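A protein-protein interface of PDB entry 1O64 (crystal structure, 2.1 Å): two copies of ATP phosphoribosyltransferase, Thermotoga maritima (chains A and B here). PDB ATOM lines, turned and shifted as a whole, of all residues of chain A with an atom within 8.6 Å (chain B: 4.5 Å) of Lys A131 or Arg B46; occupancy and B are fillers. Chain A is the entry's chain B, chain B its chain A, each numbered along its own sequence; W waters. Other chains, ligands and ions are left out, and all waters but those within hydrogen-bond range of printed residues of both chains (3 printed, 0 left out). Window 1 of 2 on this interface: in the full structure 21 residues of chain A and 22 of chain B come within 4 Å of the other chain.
Water W2 bridges the side-chain hydroxyl (OG) of Ser A133 (2.6 Å) and the guanidinium group (NH2) of Arg B46 (3.3 Å).
Water W3 lies within hydrogen-bond range of the side-chain carboxylate (OD1) of Asp B49 (2.6 Å), the backbone carbonyl oxygen (O) of Gly A132 (2.7 Å) and the backbone NH (N) of Arg B46 (3.1 Å).
Water W1 lies within hydrogen-bond range of OD2 of Asp B49 and O of Pro A129.
Among the printed residues, merely in contact across the chains: Leu A130 with Asp B49 (3.3 Å), Lys A131 with Arg B46 (3.8 Å), Gly A132 with Arg B46 (3.5 Å), Gly A132 with Asp B49 (3.6 Å), Ser A133 with Lys B9 (3.6 Å) and Leu A136 with Val B45 (3.5 Å).
O of Val B45 lies within hydrogen-bond range of N of Lys B9, at 2.8 Å.
The backbone NH (N) of Leu A130 lies within hydrogen-bond range of the backbone carbonyl oxygen (O) of Thr A108.
No position is printed for both chains.
The side-chain carboxylate of Asp B49 is in hydrogen-bond range of the backbone NH of Lys A131.
Of chain B, only Arg B46 (3.8 Å) and Asp B49 (2.9 Å) come within 4 Å of Lys A131.
Arg B46 touches two residues of chain A.
Of the printed residues of chain A, Asp B49 touches Leu A130, Lys A131 and Gly A132.
Of the printed residues of chain B, Ser A133 touches Lys B9 (3.6 Å).
Of the printed residues of chain B, Leu A136 touches Val B45 (3.5 Å).
Of the printed residues of chain A, Lys B9 touches Ser A133 (3.6 Å).
Thr A108 touches none of the printed residues of chain B.
Ala A107 touches none of the printed residues of chain B.
The nearest residue of chain A that does not touch Arg B46 is Ser A133 (4.9 Å).
Of the 14 printed residues of chain A, 5 touch a printed residue of chain B.
Hydrophobic or aromatic side chains of chain A that line the printed part of chain B: Leu A130 and Leu A136.
Among the printed residues, no Asp or Glu carboxylate lies within 4 Å of a Lys or Arg side-chain nitrogen of the other chain.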
ATOM      1  N   ALA A 107      -3.853 -14.872   4.365  1.00  0.00           N
ATOM      2  CA  ALA A 107      -3.768 -13.686   3.513  1.00  0.00           C
ATOM      3  C   ALA A 107      -2.523 -12.887   3.918  1.00  0.00           C
ATOM      4  O   ALA A 107      -2.151 -12.825   5.095  1.00  0.00           O
ATOM      5  CB  ALA A 107      -5.011 -12.824   3.632  1.00  0.00           C
ATOM      6  N   THR A 108      -1.882 -12.203   2.952  1.00  0.00           N
ATOM      7  CA  THR A 108      -0.672 -11.472   3.346  1.00  0.00           C
ATOM      8  C   THR A 108      -0.193 -10.532   2.243  1.00  0.00           C
ATOM      9  O   THR A 108      -0.532 -10.724   1.083  1.00  0.00           O
ATOM     10  CB  THR A 108       0.459 -12.479   3.648  1.00  0.00           C
ATOM     11  OG1 THR A 108       1.628 -11.812   4.128  1.00  0.00           O
ATOM     12  CG2 THR A 108       0.857 -13.295   2.405  1.00  0.00           C
ATOM     13  N   LYS A 109       0.635  -9.573   2.627  1.00  0.00           N
ATOM     14  CA  LYS A 109       1.283  -8.679   1.662  1.00  0.00           C
ATOM     15  C   LYS A 109       2.688  -9.215   1.367  1.00  0.00           C
ATOM     16  O   LYS A 109       3.430  -8.750   0.497  1.00  0.00           O
ATOM     17  CB  LYS A 109       1.417  -7.261   2.214  1.00  0.00           C
ATOM     18  CG  LYS A 109       0.086  -6.533   2.231  1.00  0.00           C
ATOM     19  CD  LYS A 109       0.091  -5.331   3.147  1.00  0.00           C
ATOM     20  CE  LYS A 109       1.262  -4.399   2.877  1.00  0.00           C
ATOM     21  NZ  LYS A 109       1.480  -3.545   4.096  1.00  0.00           N
ATOM     22  N   PHE A 110       3.051 -10.275   2.105  1.00  0.00           N
ATOM     23  CA  PHE A 110       4.347 -10.933   2.024  1.00  0.00           C
ATOM     24  C   PHE A 110       4.237 -12.424   1.725  1.00  0.00           C
ATOM     25  O   PHE A 110       4.482 -13.291   2.559  1.00  0.00           O
ATOM     26  CB  PHE A 110       5.072 -10.710   3.368  1.00  0.00           C
ATOM     27  CG  PHE A 110       5.020  -9.295   3.867  1.00  0.00           C
ATOM     28  CD1 PHE A 110       5.931  -8.354   3.387  1.00  0.00           C
ATOM     29  CD2 PHE A 110       4.058  -8.891   4.773  1.00  0.00           C
ATOM     30  CE1 PHE A 110       5.872  -7.037   3.803  1.00  0.00           C
ATOM     31  CE2 PHE A 110       4.003  -7.571   5.194  1.00  0.00           C
ATOM     32  CZ  PHE A 110       4.909  -6.642   4.723  1.00  0.00           C
ATOM     33  N   PRO A 111       3.891 -12.801   0.494  1.00  0.00           N
ATOM     34  CA  PRO A 111       3.719 -14.180   0.095  1.00  0.00           C
ATOM     35  C   PRO A 111       4.966 -15.034   0.189  1.00  0.00           C
ATOM     36  O   PRO A 111       4.887 -16.189   0.682  1.00  0.00           O
ATOM     37  CB  PRO A 111       3.168 -14.111  -1.320  1.00  0.00           C
ATOM     38  CG  PRO A 111       3.577 -12.765  -1.833  1.00  0.00           C
ATOM     39  CD  PRO A 111       3.608 -11.861  -0.633  1.00  0.00           C
ATOM     40  N   ILE A 128      -2.867 -16.093   0.063  1.00  0.00           N
ATOM     41  CA  ILE A 128      -3.647 -15.092  -0.667  1.00  0.00           C
ATOM     42  C   ILE A 128      -2.980 -13.718  -0.550  1.00  0.00           C
ATOM     43  O   ILE A 128      -3.093 -13.056   0.470  1.00  0.00           O
ATOM     44  CB  ILE A 128      -5.085 -15.004  -0.124  1.00  0.00           C
ATOM     45  CG1 ILE A 128      -5.751 -16.400  -0.180  1.00  0.00           C
ATOM     46  CG2 ILE A 128      -5.943 -14.021  -0.898  1.00  0.00           C
ATOM     47  CD1 ILE A 128      -6.893 -16.560   0.786  1.00  0.00           C
ATOM     48  N   PRO A 129      -2.288 -13.292  -1.595  1.00  0.00           N
ATOM     49  CA  PRO A 129      -1.617 -12.015  -1.628  1.00  0.00           C
ATOM     50  C   PRO A 129      -2.611 -10.862  -1.618  1.00  0.00           C
ATOM     51  O   PRO A 129      -3.614 -10.884  -2.341  1.00  0.00           O
ATOM     52  CB  PRO A 129      -0.838 -11.987  -2.937  1.00  0.00           C
ATOM     53  CG  PRO A 129      -0.964 -13.334  -3.522  1.00  0.00           C
ATOM     54  CD  PRO A 129      -2.112 -14.041  -2.870  1.00  0.00           C
ATOM     55  N   LEU A 130      -2.345  -9.867  -0.796  1.00  0.00           N
ATOM     56  CA  LEU A 130      -3.191  -8.681  -0.693  1.00  0.00           C
ATOM     57  C   LEU A 130      -2.243  -7.469  -0.705  1.00  0.00           C
ATOM     58  O   LEU A 130      -1.034  -7.661  -0.495  1.00  0.00           O
ATOM     59  CB  LEU A 130      -4.038  -8.698   0.574  1.00  0.00           C
ATOM     60  CG  LEU A 130      -5.192  -9.722   0.648  1.00  0.00           C
ATOM     61  CD1 LEU A 130      -5.921  -9.612   1.985  1.00  0.00           C
ATOM     62  CD2 LEU A 130      -6.175  -9.516  -0.502  1.00  0.00           C
ATOM     63  N   LYS A 131      -2.762  -6.291  -0.997  1.00  0.00           N
ATOM     64  CA  LYS A 131      -1.932  -5.095  -1.064  1.00  0.00           C
ATOM     65  C   LYS A 131      -2.042  -4.259   0.202  1.00  0.00           C
ATOM     66  O   LYS A 131      -1.226  -3.365   0.398  1.00  0.00           O
ATOM     67  CB  LYS A 131      -2.338  -4.228  -2.262  1.00  0.00           C
ATOM     68  CG  LYS A 131      -2.263  -4.900  -3.604  1.00  0.00           C
ATOM     69  CD  LYS A 131      -0.830  -5.225  -4.019  1.00  0.00           C
ATOM     70  CE  LYS A 131      -0.826  -5.691  -5.471  1.00  0.00           C
ATOM     71  NZ  LYS A 131       0.533  -5.641  -6.066  1.00  0.00           N
ATOM     72  N   GLY A 132      -3.086  -4.475   1.015  1.00  0.00           N
ATOM     73  CA  GLY A 132      -3.201  -3.677   2.249  1.00  0.00           C
ATOM     74  C   GLY A 132      -4.445  -4.071   3.022  1.00  0.00           C
ATOM     75  O   GLY A 132      -5.206  -4.957   2.601  1.00  0.00           O
ATOM     76  N   SER A 133      -4.642  -3.478   4.193  1.00  0.00           N
ATOM     77  CA  SER A 133      -5.794  -3.820   5.034  1.00  0.00           C
ATOM     78  C   SER A 133      -5.970  -5.332   5.116  1.00  0.00           C
ATOM     79  O   SER A 133      -7.072  -5.894   4.980  1.00  0.00           O
ATOM     80  CB  SER A 133      -7.060  -3.185   4.440  1.00  0.00           C
ATOM     81  OG  SER A 133      -6.816  -1.803   4.235  1.00  0.00           O
ATOM     82  N   VAL A 134      -4.858  -6.013   5.394  1.00  0.00           N
ATOM     83  CA  VAL A 134      -4.842  -7.465   5.479  1.00  0.00           C
ATOM     84  C   VAL A 134      -5.724  -7.991   6.591  1.00  0.00           C
ATOM     85  O   VAL A 134      -6.325  -9.073   6.472  1.00  0.00           O
ATOM     86  CB  VAL A 134      -3.390  -7.946   5.570  1.00  0.00           C
ATOM     87  CG1 VAL A 134      -3.278  -9.435   5.831  1.00  0.00           C
ATOM     88  CG2 VAL A 134      -2.671  -7.619   4.225  1.00  0.00           C
ATOM     89  N   LEU A 136      -8.673  -7.409   7.256  1.00  0.00           N
ATOM     90  CA  LEU A 136     -10.032  -7.621   6.800  1.00  0.00           C
ATOM     91  C   LEU A 136     -10.255  -9.060   6.337  1.00  0.00           C
ATOM     92  O   LEU A 136     -11.358  -9.601   6.486  1.00  0.00           O
ATOM     93  CB  LEU A 136     -10.373  -6.645   5.670  1.00  0.00           C
ATOM     94  CG  LEU A 136     -11.778  -6.698   5.068  1.00  0.00           C
ATOM     95  CD1 LEU A 136     -12.826  -6.422   6.166  1.00  0.00           C
ATOM     96  CD2 LEU A 136     -11.972  -5.705   3.951  1.00  0.00           C
ATOM     97  N   ASP A 148       1.420 -10.514   8.761  1.00  0.00           N
ATOM     98  CA  ASP A 148       1.477  -9.082   8.508  1.00  0.00           C
ATOM     99  C   ASP A 148       2.309  -8.411   9.594  1.00  0.00           C
ATOM    100  O   ASP A 148       2.677  -9.043  10.576  1.00  0.00           O
ATOM    101  CB  ASP A 148       0.031  -8.537   8.531  1.00  0.00           C
ATOM    102  CG  ASP A 148      -0.116  -7.170   7.883  1.00  0.00           C
ATOM    103  OD1 ASP A 148       0.849  -6.721   7.217  1.00  0.00           O
ATOM    104  OD2 ASP A 148      -1.185  -6.537   8.022  1.00  0.00           O
ATOM    105  N   LYS B   9     -10.671   1.368  -2.242  1.00  0.00           N
ATOM    106  CA  LYS B   9     -10.284   2.534  -1.446  1.00  0.00           C
ATOM    107  C   LYS B   9      -9.487   3.453  -2.373  1.00  0.00           C
ATOM    108  O   LYS B   9      -8.948   2.977  -3.375  1.00  0.00           O
ATOM    109  CB  LYS B   9      -9.372   2.141  -0.281  1.00  0.00           C
ATOM    110  CG  LYS B   9     -10.067   1.501   0.901  1.00  0.00           C
ATOM    111  CD  LYS B   9     -10.135   2.474   2.077  1.00  0.00           C
ATOM    112  CE  LYS B   9      -9.103   2.119   3.136  1.00  0.00           C
ATOM    113  NZ  LYS B   9      -9.308   0.731   3.651  1.00  0.00           N
ATOM    114  N   VAL B  45     -11.434  -2.236   0.368  1.00  0.00           N
ATOM    115  CA  VAL B  45     -10.142  -2.851   0.122  1.00  0.00           C
ATOM    116  C   VAL B  45      -9.296  -2.084  -0.886  1.00  0.00           C
ATOM    117  O   VAL B  45      -9.802  -1.192  -1.580  1.00  0.00           O
ATOM    118  CB  VAL B  45     -10.310  -4.305  -0.388  1.00  0.00           C
ATOM    119  CG1 VAL B  45     -11.135  -5.144   0.570  1.00  0.00           C
ATOM    120  CG2 VAL B  45     -10.941  -4.310  -1.783  1.00  0.00           C
ATOM    121  N   ARG B  46      -8.012  -2.429  -0.942  1.00  0.00           N
ATOM    122  CA  ARG B  46      -7.152  -1.778  -1.971  1.00  0.00           C
ATOM    123  C   ARG B  46      -7.741  -2.162  -3.335  1.00  0.00           C
ATOM    124  O   ARG B  46      -8.223  -3.283  -3.483  1.00  0.00           O
ATOM    125  CB  ARG B  46      -5.734  -2.243  -1.845  1.00  0.00           C
ATOM    126  CG  ARG B  46      -4.964  -2.001  -0.584  1.00  0.00           C
ATOM    127  CD  ARG B  46      -4.936  -0.591  -0.077  1.00  0.00           C
ATOM    128  NE  ARG B  46      -4.868   0.435  -1.106  1.00  0.00           N
ATOM    129  CZ  ARG B  46      -5.326   1.679  -0.925  1.00  0.00           C
ATOM    130  NH1 ARG B  46      -5.244   2.558  -1.923  1.00  0.00           N
ATOM    131  NH2 ARG B  46      -5.866   2.032   0.237  1.00  0.00           N
ATOM    132  N   PRO B  47      -7.650  -1.288  -4.321  1.00  0.00           N
ATOM    133  CA  PRO B  47      -8.193  -1.486  -5.644  1.00  0.00           C
ATOM    134  C   PRO B  47      -7.826  -2.780  -6.308  1.00  0.00           C
ATOM    135  O   PRO B  47      -8.697  -3.503  -6.831  1.00  0.00           O
ATOM    136  CB  PRO B  47      -7.646  -0.291  -6.447  1.00  0.00           C
ATOM    137  CG  PRO B  47      -7.551   0.781  -5.402  1.00  0.00           C
ATOM    138  CD  PRO B  47      -7.007   0.059  -4.186  1.00  0.00           C
ATOM    139  N   PHE B  48      -6.528  -3.137  -6.269  1.00  0.00           N
ATOM    140  CA  PHE B  48      -6.069  -4.388  -6.825  1.00  0.00           C
ATOM    141  C   PHE B  48      -6.570  -5.612  -6.080  1.00  0.00           C
ATOM    142  O   PHE B  48      -6.508  -6.727  -6.636  1.00  0.00           O
ATOM    143  CB  PHE B  48      -4.522  -4.443  -6.923  1.00  0.00           C
ATOM    144  CG  PHE B  48      -4.086  -3.966  -8.291  1.00  0.00           C
ATOM    145  CD1 PHE B  48      -3.915  -2.615  -8.541  1.00  0.00           C
ATOM    146  CD2 PHE B  48      -3.929  -4.875  -9.322  1.00  0.00           C
ATOM    147  CE1 PHE B  48      -3.554  -2.165  -9.804  1.00  0.00           C
ATOM    148  CE2 PHE B  48      -3.570  -4.431 -10.586  1.00  0.00           C
ATOM    149  CZ  PHE B  48      -3.378  -3.083 -10.820  1.00  0.00           C
ATOM    150  N   ASP B  49      -7.128  -5.462  -4.895  1.00  0.00           N
ATOM    151  CA  ASP B  49      -7.633  -6.607  -4.115  1.00  0.00           C
ATOM    152  C   ASP B  49      -9.107  -6.848  -4.394  1.00  0.00           C
ATOM    153  O   ASP B  49      -9.709  -7.856  -3.971  1.00  0.00           O
ATOM    154  CB  ASP B  49      -7.381  -6.342  -2.640  1.00  0.00           C
ATOM    155  CG  ASP B  49      -5.919  -6.391  -2.250  1.00  0.00           C
ATOM    156  OD1 ASP B  49      -5.569  -5.752  -1.250  1.00  0.00           O
ATOM    157  OD2 ASP B  49      -5.103  -7.075  -2.917  1.00  0.00           O
ATOM    158  N   VAL B  50      -9.728  -5.956  -5.169  1.00  0.00           N
ATOM    159  CA  VAL B  50     -11.142  -6.128  -5.511  1.00  0.00           C
ATOM    160  C   VAL B  50     -11.398  -7.427  -6.250  1.00  0.00           C
ATOM    161  O   VAL B  50     -12.231  -8.234  -5.818  1.00  0.00           O
ATOM    162  CB  VAL B  50     -11.714  -4.919  -6.275  1.00  0.00           C
ATOM    163  CG1 VAL B  50     -13.081  -5.284  -6.874  1.00  0.00           C
ATOM    164  CG2 VAL B  50     -11.813  -3.754  -5.303  1.00  0.00           C
HETATM  165  O   HOH W   1      -4.868  -9.357  -4.323  1.00  0.00           O
HETATM  166  O   HOH W   2      -5.788   0.178   2.981  1.00  0.00           O
HETATM  167  O   HOH W   3      -7.062  -4.863   0.651  1.00  0.00           O
